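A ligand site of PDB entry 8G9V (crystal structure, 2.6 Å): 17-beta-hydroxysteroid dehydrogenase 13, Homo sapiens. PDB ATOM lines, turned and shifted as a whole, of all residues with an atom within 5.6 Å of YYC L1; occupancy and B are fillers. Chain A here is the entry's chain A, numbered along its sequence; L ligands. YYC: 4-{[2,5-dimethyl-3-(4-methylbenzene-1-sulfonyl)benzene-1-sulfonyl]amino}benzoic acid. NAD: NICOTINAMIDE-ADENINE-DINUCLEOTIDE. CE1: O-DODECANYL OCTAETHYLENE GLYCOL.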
ATOM      1  N   ALA A 172     -24.326  -4.595   2.512  1.00  0.00           N
ATOM      2  CA  ALA A 172     -24.826  -4.108   3.786  1.00  0.00           C
ATOM      3  C   ALA A 172     -24.955  -5.315   4.786  1.00  0.00           C
ATOM      4  O   ALA A 172     -23.902  -5.911   5.012  1.00  0.00           O
ATOM      5  CB  ALA A 172     -26.109  -3.242   3.585  1.00  0.00           C
ATOM      6  N   SER A 173     -26.144  -5.720   5.330  1.00  0.00           N
ATOM      7  CA  SER A 173     -26.349  -6.783   6.323  1.00  0.00           C
ATOM      8  C   SER A 173     -27.822  -6.781   6.757  1.00  0.00           C
ATOM      9  O   SER A 173     -28.525  -5.789   6.536  1.00  0.00           O
ATOM     10  CB  SER A 173     -25.489  -6.492   7.546  1.00  0.00           C
ATOM     11  OG  SER A 173     -25.724  -7.390   8.617  1.00  0.00           O
ATOM     12  N   VAL A 174     -28.295  -7.858   7.436  1.00  0.00           N
ATOM     13  CA  VAL A 174     -29.657  -7.813   8.049  1.00  0.00           C
ATOM     14  C   VAL A 174     -29.696  -6.723   9.131  1.00  0.00           C
ATOM     15  O   VAL A 174     -30.767  -6.197   9.413  1.00  0.00           O
ATOM     16  CB  VAL A 174     -30.146  -9.142   8.649  1.00  0.00           C
ATOM     17  CG1 VAL A 174     -30.732 -10.022   7.582  1.00  0.00           C
ATOM     18  CG2 VAL A 174     -29.040  -9.852   9.393  1.00  0.00           C
ATOM     19  N   CYS A 175     -28.525  -6.365   9.720  1.00  0.00           N
ATOM     20  CA  CYS A 175     -28.341  -5.274  10.656  1.00  0.00           C
ATOM     21  C   CYS A 175     -28.598  -3.884  10.052  1.00  0.00           C
ATOM     22  O   CYS A 175     -28.560  -2.915  10.781  1.00  0.00           O
ATOM     23  CB  CYS A 175     -26.963  -5.352  11.287  1.00  0.00           C
ATOM     24  SG  CYS A 175     -26.714  -6.833  12.285  1.00  0.00           S
ATOM     25  N   GLU A 178     -32.635  -4.156  10.894  1.00  0.00           N
ATOM     26  CA  GLU A 178     -33.020  -4.198  12.300  1.00  0.00           C
ATOM     27  C   GLU A 178     -31.772  -4.052  13.197  1.00  0.00           C
ATOM     28  O   GLU A 178     -30.734  -4.642  12.903  1.00  0.00           O
ATOM     29  CB  GLU A 178     -33.807  -5.462  12.629  1.00  0.00           C
ATOM     30  CG  GLU A 178     -34.421  -5.478  14.036  1.00  0.00           C
ATOM     31  CD  GLU A 178     -35.146  -4.215  14.499  1.00  0.00           C
ATOM     32  OE1 GLU A 178     -36.008  -3.698  13.747  1.00  0.00           O
ATOM     33  OE2 GLU A 178     -34.836  -3.726  15.609  1.00  0.00           O
ATOM     34  N   GLY A 179     -31.881  -3.251  14.243  1.00  0.00           N
ATOM     35  CA  GLY A 179     -30.824  -3.056  15.222  1.00  0.00           C
ATOM     36  C   GLY A 179     -30.757  -4.201  16.218  1.00  0.00           C
ATOM     37  O   GLY A 179     -31.783  -4.748  16.627  1.00  0.00           O
ATOM     38  N   ILE A 180     -29.536  -4.612  16.566  1.00  0.00           N
ATOM     39  CA  ILE A 180     -29.324  -5.687  17.490  1.00  0.00           C
ATOM     40  C   ILE A 180     -28.376  -5.220  18.634  1.00  0.00           C
ATOM     41  O   ILE A 180     -27.565  -4.308  18.444  1.00  0.00           O
ATOM     42  CB  ILE A 180     -28.915  -7.025  16.811  1.00  0.00           C
ATOM     43  CG1 ILE A 180     -27.678  -6.947  15.922  1.00  0.00           C
ATOM     44  CG2 ILE A 180     -30.076  -7.650  16.081  1.00  0.00           C
ATOM     45  CD1 ILE A 180     -27.162  -8.283  15.579  1.00  0.00           C
ATOM     46  N   LEU A 183     -24.067  -4.033  19.107  1.00  0.00           N
ATOM     47  CA  LEU A 183     -23.638  -3.725  17.753  1.00  0.00           C
ATOM     48  C   LEU A 183     -24.340  -2.434  17.263  1.00  0.00           C
ATOM     49  O   LEU A 183     -24.606  -2.324  16.071  1.00  0.00           O
ATOM     50  CB  LEU A 183     -24.004  -4.886  16.802  1.00  0.00           C
ATOM     51  CG  LEU A 183     -23.212  -6.169  16.890  1.00  0.00           C
ATOM     52  CD1 LEU A 183     -23.698  -7.151  15.876  1.00  0.00           C
ATOM     53  CD2 LEU A 183     -21.754  -5.925  16.680  1.00  0.00           C
ATOM     54  N   TYR A 186     -22.478  -0.421  14.526  1.00  0.00           N
ATOM     55  CA  TYR A 186     -22.409  -1.253  13.338  1.00  0.00           C
ATOM     56  C   TYR A 186     -23.749  -1.285  12.602  1.00  0.00           C
ATOM     57  O   TYR A 186     -23.794  -1.131  11.379  1.00  0.00           O
ATOM     58  CB  TYR A 186     -21.965  -2.670  13.704  1.00  0.00           C
ATOM     59  CG  TYR A 186     -21.964  -3.609  12.521  1.00  0.00           C
ATOM     60  CD1 TYR A 186     -20.925  -3.600  11.599  1.00  0.00           C
ATOM     61  CD2 TYR A 186     -23.001  -4.519  12.330  1.00  0.00           C
ATOM     62  CE1 TYR A 186     -20.919  -4.461  10.521  1.00  0.00           C
ATOM     63  CE2 TYR A 186     -23.017  -5.375  11.254  1.00  0.00           C
ATOM     64  CZ  TYR A 186     -21.969  -5.354  10.351  1.00  0.00           C
ATOM     65  OH  TYR A 186     -21.960  -6.215   9.298  1.00  0.00           O
ATOM     66  N   PRO A 219     -26.922 -10.198   4.115  1.00  0.00           N
ATOM     67  CA  PRO A 219     -26.925 -11.545   4.700  1.00  0.00           C
ATOM     68  C   PRO A 219     -27.067 -11.561   6.217  1.00  0.00           C
ATOM     69  O   PRO A 219     -26.821 -10.554   6.884  1.00  0.00           O
ATOM     70  CB  PRO A 219     -25.561 -12.129   4.265  1.00  0.00           C
ATOM     71  CG  PRO A 219     -24.761 -10.969   3.719  1.00  0.00           C
ATOM     72  CD  PRO A 219     -25.540  -9.708   3.950  1.00  0.00           C
ATOM     73  N   VAL A 220     -27.461 -12.735   6.757  1.00  0.00           N
ATOM     74  CA  VAL A 220     -27.516 -12.958   8.211  1.00  0.00           C
ATOM     75  C   VAL A 220     -26.083 -13.351   8.652  1.00  0.00           C
ATOM     76  O   VAL A 220     -25.154 -13.228   7.848  1.00  0.00           O
ATOM     77  CB  VAL A 220     -28.607 -14.006   8.583  1.00  0.00           C
ATOM     78  CG1 VAL A 220     -29.996 -13.486   8.290  1.00  0.00           C
ATOM     79  CG2 VAL A 220     -28.337 -15.328   7.898  1.00  0.00           C
ATOM     80  N   PHE A 221     -25.860 -13.789   9.913  1.00  0.00           N
ATOM     81  CA  PHE A 221     -24.527 -14.162  10.370  1.00  0.00           C
ATOM     82  C   PHE A 221     -23.867 -15.218   9.467  1.00  0.00           C
ATOM     83  O   PHE A 221     -24.415 -16.298   9.275  1.00  0.00           O
ATOM     84  CB  PHE A 221     -24.567 -14.625  11.830  1.00  0.00           C
ATOM     85  CG  PHE A 221     -23.213 -15.038  12.343  1.00  0.00           C
ATOM     86  CD1 PHE A 221     -22.325 -14.098  12.827  1.00  0.00           C
ATOM     87  CD2 PHE A 221     -22.805 -16.362  12.284  1.00  0.00           C
ATOM     88  CE1 PHE A 221     -21.071 -14.496  13.285  1.00  0.00           C
ATOM     89  CE2 PHE A 221     -21.546 -16.749  12.712  1.00  0.00           C
ATOM     90  CZ  PHE A 221     -20.689 -15.809  13.216  1.00  0.00           C
ATOM     91  N   PHE A 226     -15.555 -12.486  11.034  1.00  0.00           N
ATOM     92  CA  PHE A 226     -15.885 -11.061  11.148  1.00  0.00           C
ATOM     93  C   PHE A 226     -16.348 -10.778  12.598  1.00  0.00           C
ATOM     94  O   PHE A 226     -15.849  -9.854  13.258  1.00  0.00           O
ATOM     95  CB  PHE A 226     -16.988 -10.712  10.118  1.00  0.00           C
ATOM     96  CG  PHE A 226     -17.318  -9.245   9.993  1.00  0.00           C
ATOM     97  CD1 PHE A 226     -16.448  -8.372   9.374  1.00  0.00           C
ATOM     98  CD2 PHE A 226     -18.504  -8.738  10.478  1.00  0.00           C
ATOM     99  CE1 PHE A 226     -16.745  -7.024   9.276  1.00  0.00           C
ATOM    100  CE2 PHE A 226     -18.805  -7.400  10.352  1.00  0.00           C
ATOM    101  CZ  PHE A 226     -17.906  -6.546   9.788  1.00  0.00           C
ATOM    102  N   THR A 227     -17.277 -11.604  13.087  1.00  0.00           N
ATOM    103  CA  THR A 227     -17.739 -11.605  14.468  1.00  0.00           C
ATOM    104  C   THR A 227     -17.524 -13.036  14.984  1.00  0.00           C
ATOM    105  O   THR A 227     -17.597 -13.972  14.167  1.00  0.00           O
ATOM    106  CB  THR A 227     -19.184 -11.068  14.633  1.00  0.00           C
ATOM    107  OG1 THR A 227     -20.022 -11.447  13.533  1.00  0.00           O
ATOM    108  CG2 THR A 227     -19.218  -9.562  14.773  1.00  0.00           C
ATOM    109  N   TRP A 235     -27.331 -21.691  17.072  1.00  0.00           N
ATOM    110  CA  TRP A 235     -28.223 -20.952  16.175  1.00  0.00           C
ATOM    111  C   TRP A 235     -27.759 -21.355  14.748  1.00  0.00           C
ATOM    112  O   TRP A 235     -26.572 -21.633  14.546  1.00  0.00           O
ATOM    113  CB  TRP A 235     -28.049 -19.431  16.418  1.00  0.00           C
ATOM    114  CG  TRP A 235     -28.790 -18.525  15.480  1.00  0.00           C
ATOM    115  CD1 TRP A 235     -28.343 -18.022  14.292  1.00  0.00           C
ATOM    116  CD2 TRP A 235     -30.110 -17.996  15.668  1.00  0.00           C
ATOM    117  NE1 TRP A 235     -29.320 -17.245  13.708  1.00  0.00           N
ATOM    118  CE2 TRP A 235     -30.412 -17.213  14.537  1.00  0.00           C
ATOM    119  CE3 TRP A 235     -31.067 -18.117  16.677  1.00  0.00           C
ATOM    120  CZ2 TRP A 235     -31.624 -16.544  14.394  1.00  0.00           C
ATOM    121  CZ3 TRP A 235     -32.258 -17.452  16.531  1.00  0.00           C
ATOM    122  CH2 TRP A 235     -32.530 -16.671  15.413  1.00  0.00           C
ATOM    123  N   ILE A 264     -35.552 -14.073   4.493  1.00  0.00           N
ATOM    124  CA  ILE A 264     -35.469 -13.260   5.713  1.00  0.00           C
ATOM    125  C   ILE A 264     -36.238 -11.932   5.580  1.00  0.00           C
ATOM    126  O   ILE A 264     -36.443 -11.283   6.595  1.00  0.00           O
ATOM    127  CB  ILE A 264     -34.046 -13.050   6.289  1.00  0.00           C
ATOM    128  CG1 ILE A 264     -33.272 -12.081   5.412  1.00  0.00           C
ATOM    129  CG2 ILE A 264     -33.355 -14.416   6.534  1.00  0.00           C
ATOM    130  CD1 ILE A 264     -31.780 -12.239   5.320  1.00  0.00           C
ATOM    131  N   PHE A 267     -39.352 -12.675   7.595  1.00  0.00           N
ATOM    132  CA  PHE A 267     -39.022 -12.587   9.022  1.00  0.00           C
ATOM    133  C   PHE A 267     -39.023 -11.150   9.501  1.00  0.00           C
ATOM    134  O   PHE A 267     -39.579 -10.868  10.575  1.00  0.00           O
ATOM    135  CB  PHE A 267     -37.665 -13.229   9.334  1.00  0.00           C
ATOM    136  CG  PHE A 267     -37.760 -14.716   9.447  1.00  0.00           C
ATOM    137  CD1 PHE A 267     -38.437 -15.308  10.510  1.00  0.00           C
ATOM    138  CD2 PHE A 267     -37.196 -15.548   8.493  1.00  0.00           C
ATOM    139  CE1 PHE A 267     -38.549 -16.692  10.599  1.00  0.00           C
ATOM    140  CE2 PHE A 267     -37.306 -16.923   8.585  1.00  0.00           C
ATOM    141  CZ  PHE A 267     -37.960 -17.487   9.645  1.00  0.00           C
ATOM    142  N   LEU A 268     -38.453 -10.225   8.698  1.00  0.00           N
ATOM    143  CA  LEU A 268     -38.423  -8.815   9.059  1.00  0.00           C
ATOM    144  C   LEU A 268     -39.838  -8.258   9.130  1.00  0.00           C
ATOM    145  O   LEU A 268     -40.143  -7.514  10.055  1.00  0.00           O
ATOM    146  CB  LEU A 268     -37.548  -8.004   8.071  1.00  0.00           C
ATOM    147  CG  LEU A 268     -36.051  -8.331   8.092  1.00  0.00           C
ATOM    148  CD1 LEU A 268     -35.380  -7.868   6.806  1.00  0.00           C
ATOM    149  CD2 LEU A 268     -35.373  -7.824   9.336  1.00  0.00           C
ATOM    150  N   LEU A 274     -43.593 -11.159  16.842  1.00  0.00           N
ATOM    151  CA  LEU A 274     -42.676 -12.022  17.590  1.00  0.00           C
ATOM    152  C   LEU A 274     -43.239 -12.194  18.966  1.00  0.00           C
ATOM    153  O   LEU A 274     -43.497 -11.199  19.630  1.00  0.00           O
ATOM    154  CB  LEU A 274     -41.295 -11.377  17.698  1.00  0.00           C
ATOM    155  CG  LEU A 274     -40.236 -12.205  18.409  1.00  0.00           C
ATOM    156  CD1 LEU A 274     -40.039 -13.549  17.741  1.00  0.00           C
ATOM    157  CD2 LEU A 274     -38.916 -11.485  18.452  1.00  0.00           C
ATOM    158  N   LEU A 282     -34.451 -14.886  22.866  1.00  0.00           N
ATOM    159  CA  LEU A 282     -33.493 -14.298  21.934  1.00  0.00           C
ATOM    160  C   LEU A 282     -32.617 -13.308  22.632  1.00  0.00           C
ATOM    161  O   LEU A 282     -31.400 -13.432  22.522  1.00  0.00           O
ATOM    162  CB  LEU A 282     -34.200 -13.603  20.757  1.00  0.00           C
ATOM    163  CG  LEU A 282     -34.910 -14.487  19.779  1.00  0.00           C
ATOM    164  CD1 LEU A 282     -35.790 -13.662  18.854  1.00  0.00           C
ATOM    165  CD2 LEU A 282     -33.945 -15.369  19.047  1.00  0.00           C
HETATM  166  C4  YYC L   1     -34.579 -12.813  13.613  1.00  0.00           C
HETATM  167  C7  YYC L   1     -35.622 -15.266  12.909  1.00  0.00           C
HETATM  168  C6  YYC L   1     -34.982 -14.499  11.957  1.00  0.00           C
HETATM  169  C13 YYC L   1     -30.909  -9.736  12.575  1.00  0.00           C
HETATM  170  C16 YYC L   1     -31.065 -12.538  12.112  1.00  0.00           C
HETATM  171  C26 YYC L   1     -23.999 -10.454  12.812  1.00  0.00           C
HETATM  172  C1  YYC L   1     -36.422 -15.689  15.266  1.00  0.00           C
HETATM  173  C2  YYC L   1     -35.737 -14.830  14.225  1.00  0.00           C
HETATM  174  C3  YYC L   1     -35.208 -13.591  14.556  1.00  0.00           C
HETATM  175  C5  YYC L   1     -34.457 -13.271  12.317  1.00  0.00           C
HETATM  176  S8  YYC L   1     -33.666 -12.255  11.096  1.00  0.00           S
HETATM  177  O9  YYC L   1     -34.508 -11.111  10.864  1.00  0.00           O
HETATM  178  O10 YYC L   1     -33.321 -13.098   9.979  1.00  0.00           O
HETATM  179  C11 YYC L   1     -32.147 -11.684  11.843  1.00  0.00           C
HETATM  180  C12 YYC L   1     -32.070 -10.316  12.088  1.00  0.00           C
HETATM  181  C14 YYC L   1     -29.831 -10.569  12.848  1.00  0.00           C
HETATM  182  C15 YYC L   1     -29.903 -11.927  12.632  1.00  0.00           C
HETATM  183  C17 YYC L   1     -31.135 -14.028  11.836  1.00  0.00           C
HETATM  184  S18 YYC L   1     -28.472 -12.879  13.084  1.00  0.00           S
HETATM  185  O19 YYC L   1     -27.959 -13.505  11.902  1.00  0.00           O
HETATM  186  O20 YYC L   1     -28.850 -13.693  14.204  1.00  0.00           O
HETATM  187  N21 YYC L   1     -27.331 -11.842  13.635  1.00  0.00           N
HETATM  188  C22 YYC L   1     -26.264 -11.268  12.888  1.00  0.00           C
HETATM  189  C23 YYC L   1     -26.465 -10.763  11.611  1.00  0.00           C
HETATM  190  C24 YYC L   1     -25.467 -10.085  10.953  1.00  0.00           C
HETATM  191  C25 YYC L   1     -24.221  -9.904  11.549  1.00  0.00           C
HETATM  192  C27 YYC L   1     -25.008 -11.122  13.480  1.00  0.00           C
HETATM  193  C28 YYC L   1     -23.189  -9.034  10.916  1.00  0.00           C
HETATM  194  O29 YYC L   1     -21.998  -9.117  11.240  1.00  0.00           O
HETATM  195  O30 YYC L   1     -23.619  -8.293   9.940  1.00  0.00           O
HETATM  196  C31 YYC L   1     -30.814  -8.247  12.783  1.00  0.00           C
HETATM  197  PA  NAD L   2     -14.000 -10.800   6.789  1.00  0.00           P
HETATM  198  O1A NAD L   2     -13.780 -12.227   6.474  1.00  0.00           O
HETATM  199  O2A NAD L   2     -13.367 -10.433   8.131  1.00  0.00           O
HETATM  200  O5B NAD L   2     -13.336  -9.877   5.631  1.00  0.00           O
HETATM  201  C5B NAD L   2     -13.436  -8.446   5.615  1.00  0.00           C
HETATM  202  C4B NAD L   2     -12.232  -7.914   4.886  1.00  0.00           C
HETATM  203  O4B NAD L   2     -12.318  -6.474   4.811  1.00  0.00           O
HETATM  204  C3B NAD L   2     -10.881  -8.238   5.537  1.00  0.00           C
HETATM  205  O3B NAD L   2      -9.968  -8.861   4.638  1.00  0.00           O
HETATM  206  C2B NAD L   2     -10.369  -6.879   6.020  1.00  0.00           C
HETATM  207  O2B NAD L   2      -8.957  -6.786   6.019  1.00  0.00           O
HETATM  208  C1B NAD L   2     -11.029  -5.944   5.014  1.00  0.00           C
HETATM  209  N9A NAD L   2     -11.156  -4.563   5.463  1.00  0.00           N
HETATM  210  C8A NAD L   2     -11.570  -4.126   6.695  1.00  0.00           C
HETATM  211  N7A NAD L   2     -11.418  -2.837   6.895  1.00  0.00           N
HETATM  212  C5A NAD L   2     -10.868  -2.393   5.705  1.00  0.00           C
HETATM  213  C6A NAD L   2     -10.420  -1.117   5.288  1.00  0.00           C
HETATM  214  N6A NAD L   2     -10.439  -0.037   6.079  1.00  0.00           N
HETATM  215  N1A NAD L   2      -9.917  -1.014   4.036  1.00  0.00           N
HETATM  216  C2A NAD L   2      -9.876  -2.107   3.262  1.00  0.00           C
HETATM  217  N3A NAD L   2     -10.245  -3.353   3.555  1.00  0.00           N
HETATM  218  C4A NAD L   2     -10.726  -3.437   4.800  1.00  0.00           C
HETATM  219  O3  NAD L   2     -15.562 -10.494   6.833  1.00  0.00           O
HETATM  220  PN  NAD L   2     -16.807 -10.698   5.830  1.00  0.00           P
HETATM  221  O1N NAD L   2     -16.326 -11.184   4.513  1.00  0.00           O
HETATM  222  O2N NAD L   2     -17.864 -11.456   6.530  1.00  0.00           O
HETATM  223  O5D NAD L   2     -17.306  -9.191   5.716  1.00  0.00           O
HETATM  224  C5D NAD L   2     -17.521  -8.588   4.426  1.00  0.00           C
HETATM  225  C4D NAD L   2     -18.703  -7.649   4.500  1.00  0.00           C
HETATM  226  O4D NAD L   2     -19.919  -8.383   4.754  1.00  0.00           O
HETATM  227  C3D NAD L   2     -18.618  -6.550   5.563  1.00  0.00           C
HETATM  228  O3D NAD L   2     -19.060  -5.322   5.007  1.00  0.00           O
HETATM  229  C2D NAD L   2     -19.575  -7.056   6.645  1.00  0.00           C
HETATM  230  O2D NAD L   2     -20.127  -6.003   7.404  1.00  0.00           O
HETATM  231  C1D NAD L   2     -20.626  -7.738   5.769  1.00  0.00           C
HETATM  232  N1N NAD L   2     -21.493  -8.789   6.497  1.00  0.00           N
HETATM  233  C2N NAD L   2     -20.858  -9.733   7.214  1.00  0.00           C
HETATM  234  C3N NAD L   2     -21.572 -10.665   7.935  1.00  0.00           C
HETATM  235  C7N NAD L   2     -20.903 -11.746   8.721  1.00  0.00           C
HETATM  236  O7N NAD L   2     -21.537 -12.309   9.631  1.00  0.00           O
HETATM  237  N7N NAD L   2     -19.607 -11.959   8.509  1.00  0.00           N
HETATM  238  C4N NAD L   2     -22.963 -10.631   7.857  1.00  0.00           C
HETATM  239  C5N NAD L   2     -23.596  -9.662   7.103  1.00  0.00           C
HETATM  240  C6N NAD L   2     -22.846  -8.737   6.431  1.00  0.00           C
HETATM  241  C1  CE1 L   3     -51.656 -10.740  17.139  1.00  0.00           C
HETATM  242  C2  CE1 L   3     -50.515 -11.716  16.852  1.00  0.00           C
HETATM  243  C3  CE1 L   3     -50.977 -13.179  16.592  1.00  0.00           C
HETATM  244  C4  CE1 L   3     -50.515 -14.201  17.639  1.00  0.00           C
HETATM  245  C5  CE1 L   3     -50.148 -15.599  17.105  1.00  0.00           C
HETATM  246  C6  CE1 L   3     -48.630 -15.827  16.925  1.00  0.00           C
HETATM  247  C7  CE1 L   3     -48.202 -17.240  16.393  1.00  0.00           C
HETATM  248  C8  CE1 L   3     -46.720 -17.414  15.994  1.00  0.00           C
HETATM  249  C9  CE1 L   3     -46.063 -16.158  15.385  1.00  0.00           C
HETATM  250  C10 CE1 L   3     -44.660 -16.349  14.806  1.00  0.00           C
HETATM  251  C11 CE1 L   3     -43.842 -15.061  14.671  1.00  0.00           C
HETATM  252  C12 CE1 L   3     -42.434 -15.286  14.200  1.00  0.00           C
HETATM  253  O13 CE1 L   3     -41.821 -14.054  13.814  1.00  0.00           O
HETATM  254  C14 CE1 L   3     -40.419 -13.962  14.093  1.00  0.00           C
HETATM  255  C15 CE1 L   3     -39.896 -12.645  13.609  1.00  0.00           C
HETATM  256  O16 CE1 L   3     -38.554 -12.448  14.050  1.00  0.00           O
HETATM  257  C17 CE1 L   3     -37.923 -11.310  13.475  1.00  0.00           C
HETATM  258  C18 CE1 L   3     -37.215 -10.550  14.542  1.00  0.00           C
HETATM  259  O19 CE1 L   3     -36.078  -9.869  14.007  1.00  0.00           O
HETATM  260  C20 CE1 L   3     -35.397  -9.079  14.990  1.00  0.00           C
HETATM  261  C21 CE1 L   3     -33.910  -9.289  14.949  1.00  0.00           C
HETATM  262  O22 CE1 L   3     -33.453 -10.016  16.090  1.00  0.00           O
HETATM  263  C23 CE1 L   3     -32.770 -11.235  15.791  1.00  0.00           C
HETATM  264  C24 CE1 L   3     -31.669 -11.464  16.773  1.00  0.00           C
HETATM  265  O25 CE1 L   3     -31.137 -12.775  16.605  1.00  0.00           O
HETATM  266  C26 CE1 L   3     -31.346 -13.607  17.742  1.00  0.00           C
HETATM  267  C27 CE1 L   3     -30.318 -14.679  17.820  1.00  0.00           C
HETATM  268  O28 CE1 L   3     -29.120 -14.164  18.387  1.00  0.00           O
HETATM  269  C29 CE1 L   3     -28.004 -15.038  18.221  1.00  0.00           C
HETATM  270  C30 CE1 L   3     -27.270 -14.757  16.934  1.00  0.00           C
HETATM  271  O31 CE1 L   3     -26.047 -15.486  16.917  1.00  0.00           O
HETATM  272  C32 CE1 L   3     -25.321 -15.412  15.706  1.00  0.00           C
HETATM  273  C33 CE1 L   3     -24.476 -14.178  15.659  1.00  0.00           C
HETATM  274  O34 CE1 L   3     -23.500 -14.154  16.700  1.00  0.00           O
HETATM  275  C35 CE1 L   3     -22.612 -13.017  16.646  1.00  0.00           C
HETATM  276  C36 CE1 L   3     -23.351 -11.740  17.003  1.00  0.00           C
HETATM  277  O37 CE1 L   3     -22.591 -10.840  17.827  1.00  0.00           O
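CG2 of Val 174 touches C23 of YYC L1, at 3.5 Å. Cys 175 touches YYC L1. O of Glu 178 touches C31 of YYC L1, 3.6 Å away. Ile 180 touches YYC L1. CB of Val 220 touches O19 of YYC L1, 3.4 Å away. Phe 226 touches YYC L1. Thr 227 touches YYC L1 (OG1 to O29, 3.8 Å). NE1 of Trp 235 touches O20 of YYC L1, at 3.6 Å. Ile 264 touches YYC L1. Phe 267 touches YYC L1. CD2 of Leu 268 touches O9 of YYC L1 (3.7 Å). Hydrophobic or aromatic side chains that line YYC L1: Val 174, Ile 180, Tyr 186, Val 220, Phe 221, Phe 226, Trp 235, Ile 264, Phe 267 and Leu 268. The nearest printed residue that does not touch YYC L1 is Leu 282 (4.2 Å).
The side-chain hydroxyl (OG) of Ser 173 is in hydrogen-bond range of an oxygen (O30) of YYC L1 (2.6 Å). OH of Tyr 186 sits at hydrogen-bond distance from O30 of YYC L1, 2.7 Å away. The backbone NH of Phe 221 lies within hydrogen-bond range of an oxygen (O19) of YYC L1 (2.9 Å). An oxygen (O2D) of NAD L2 sits at hydrogen-bond distance from the side-chain hydroxyl (OH) of Tyr 186, 2.6 Å away.
OG of Ser 173 sits close to N of Cys 175 (3.2 Å). The backbone carbonyl oxygen (O) of Pro 219 lies within hydrogen-bond range of the backbone NH (N) of Val 174 (3.1 Å).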
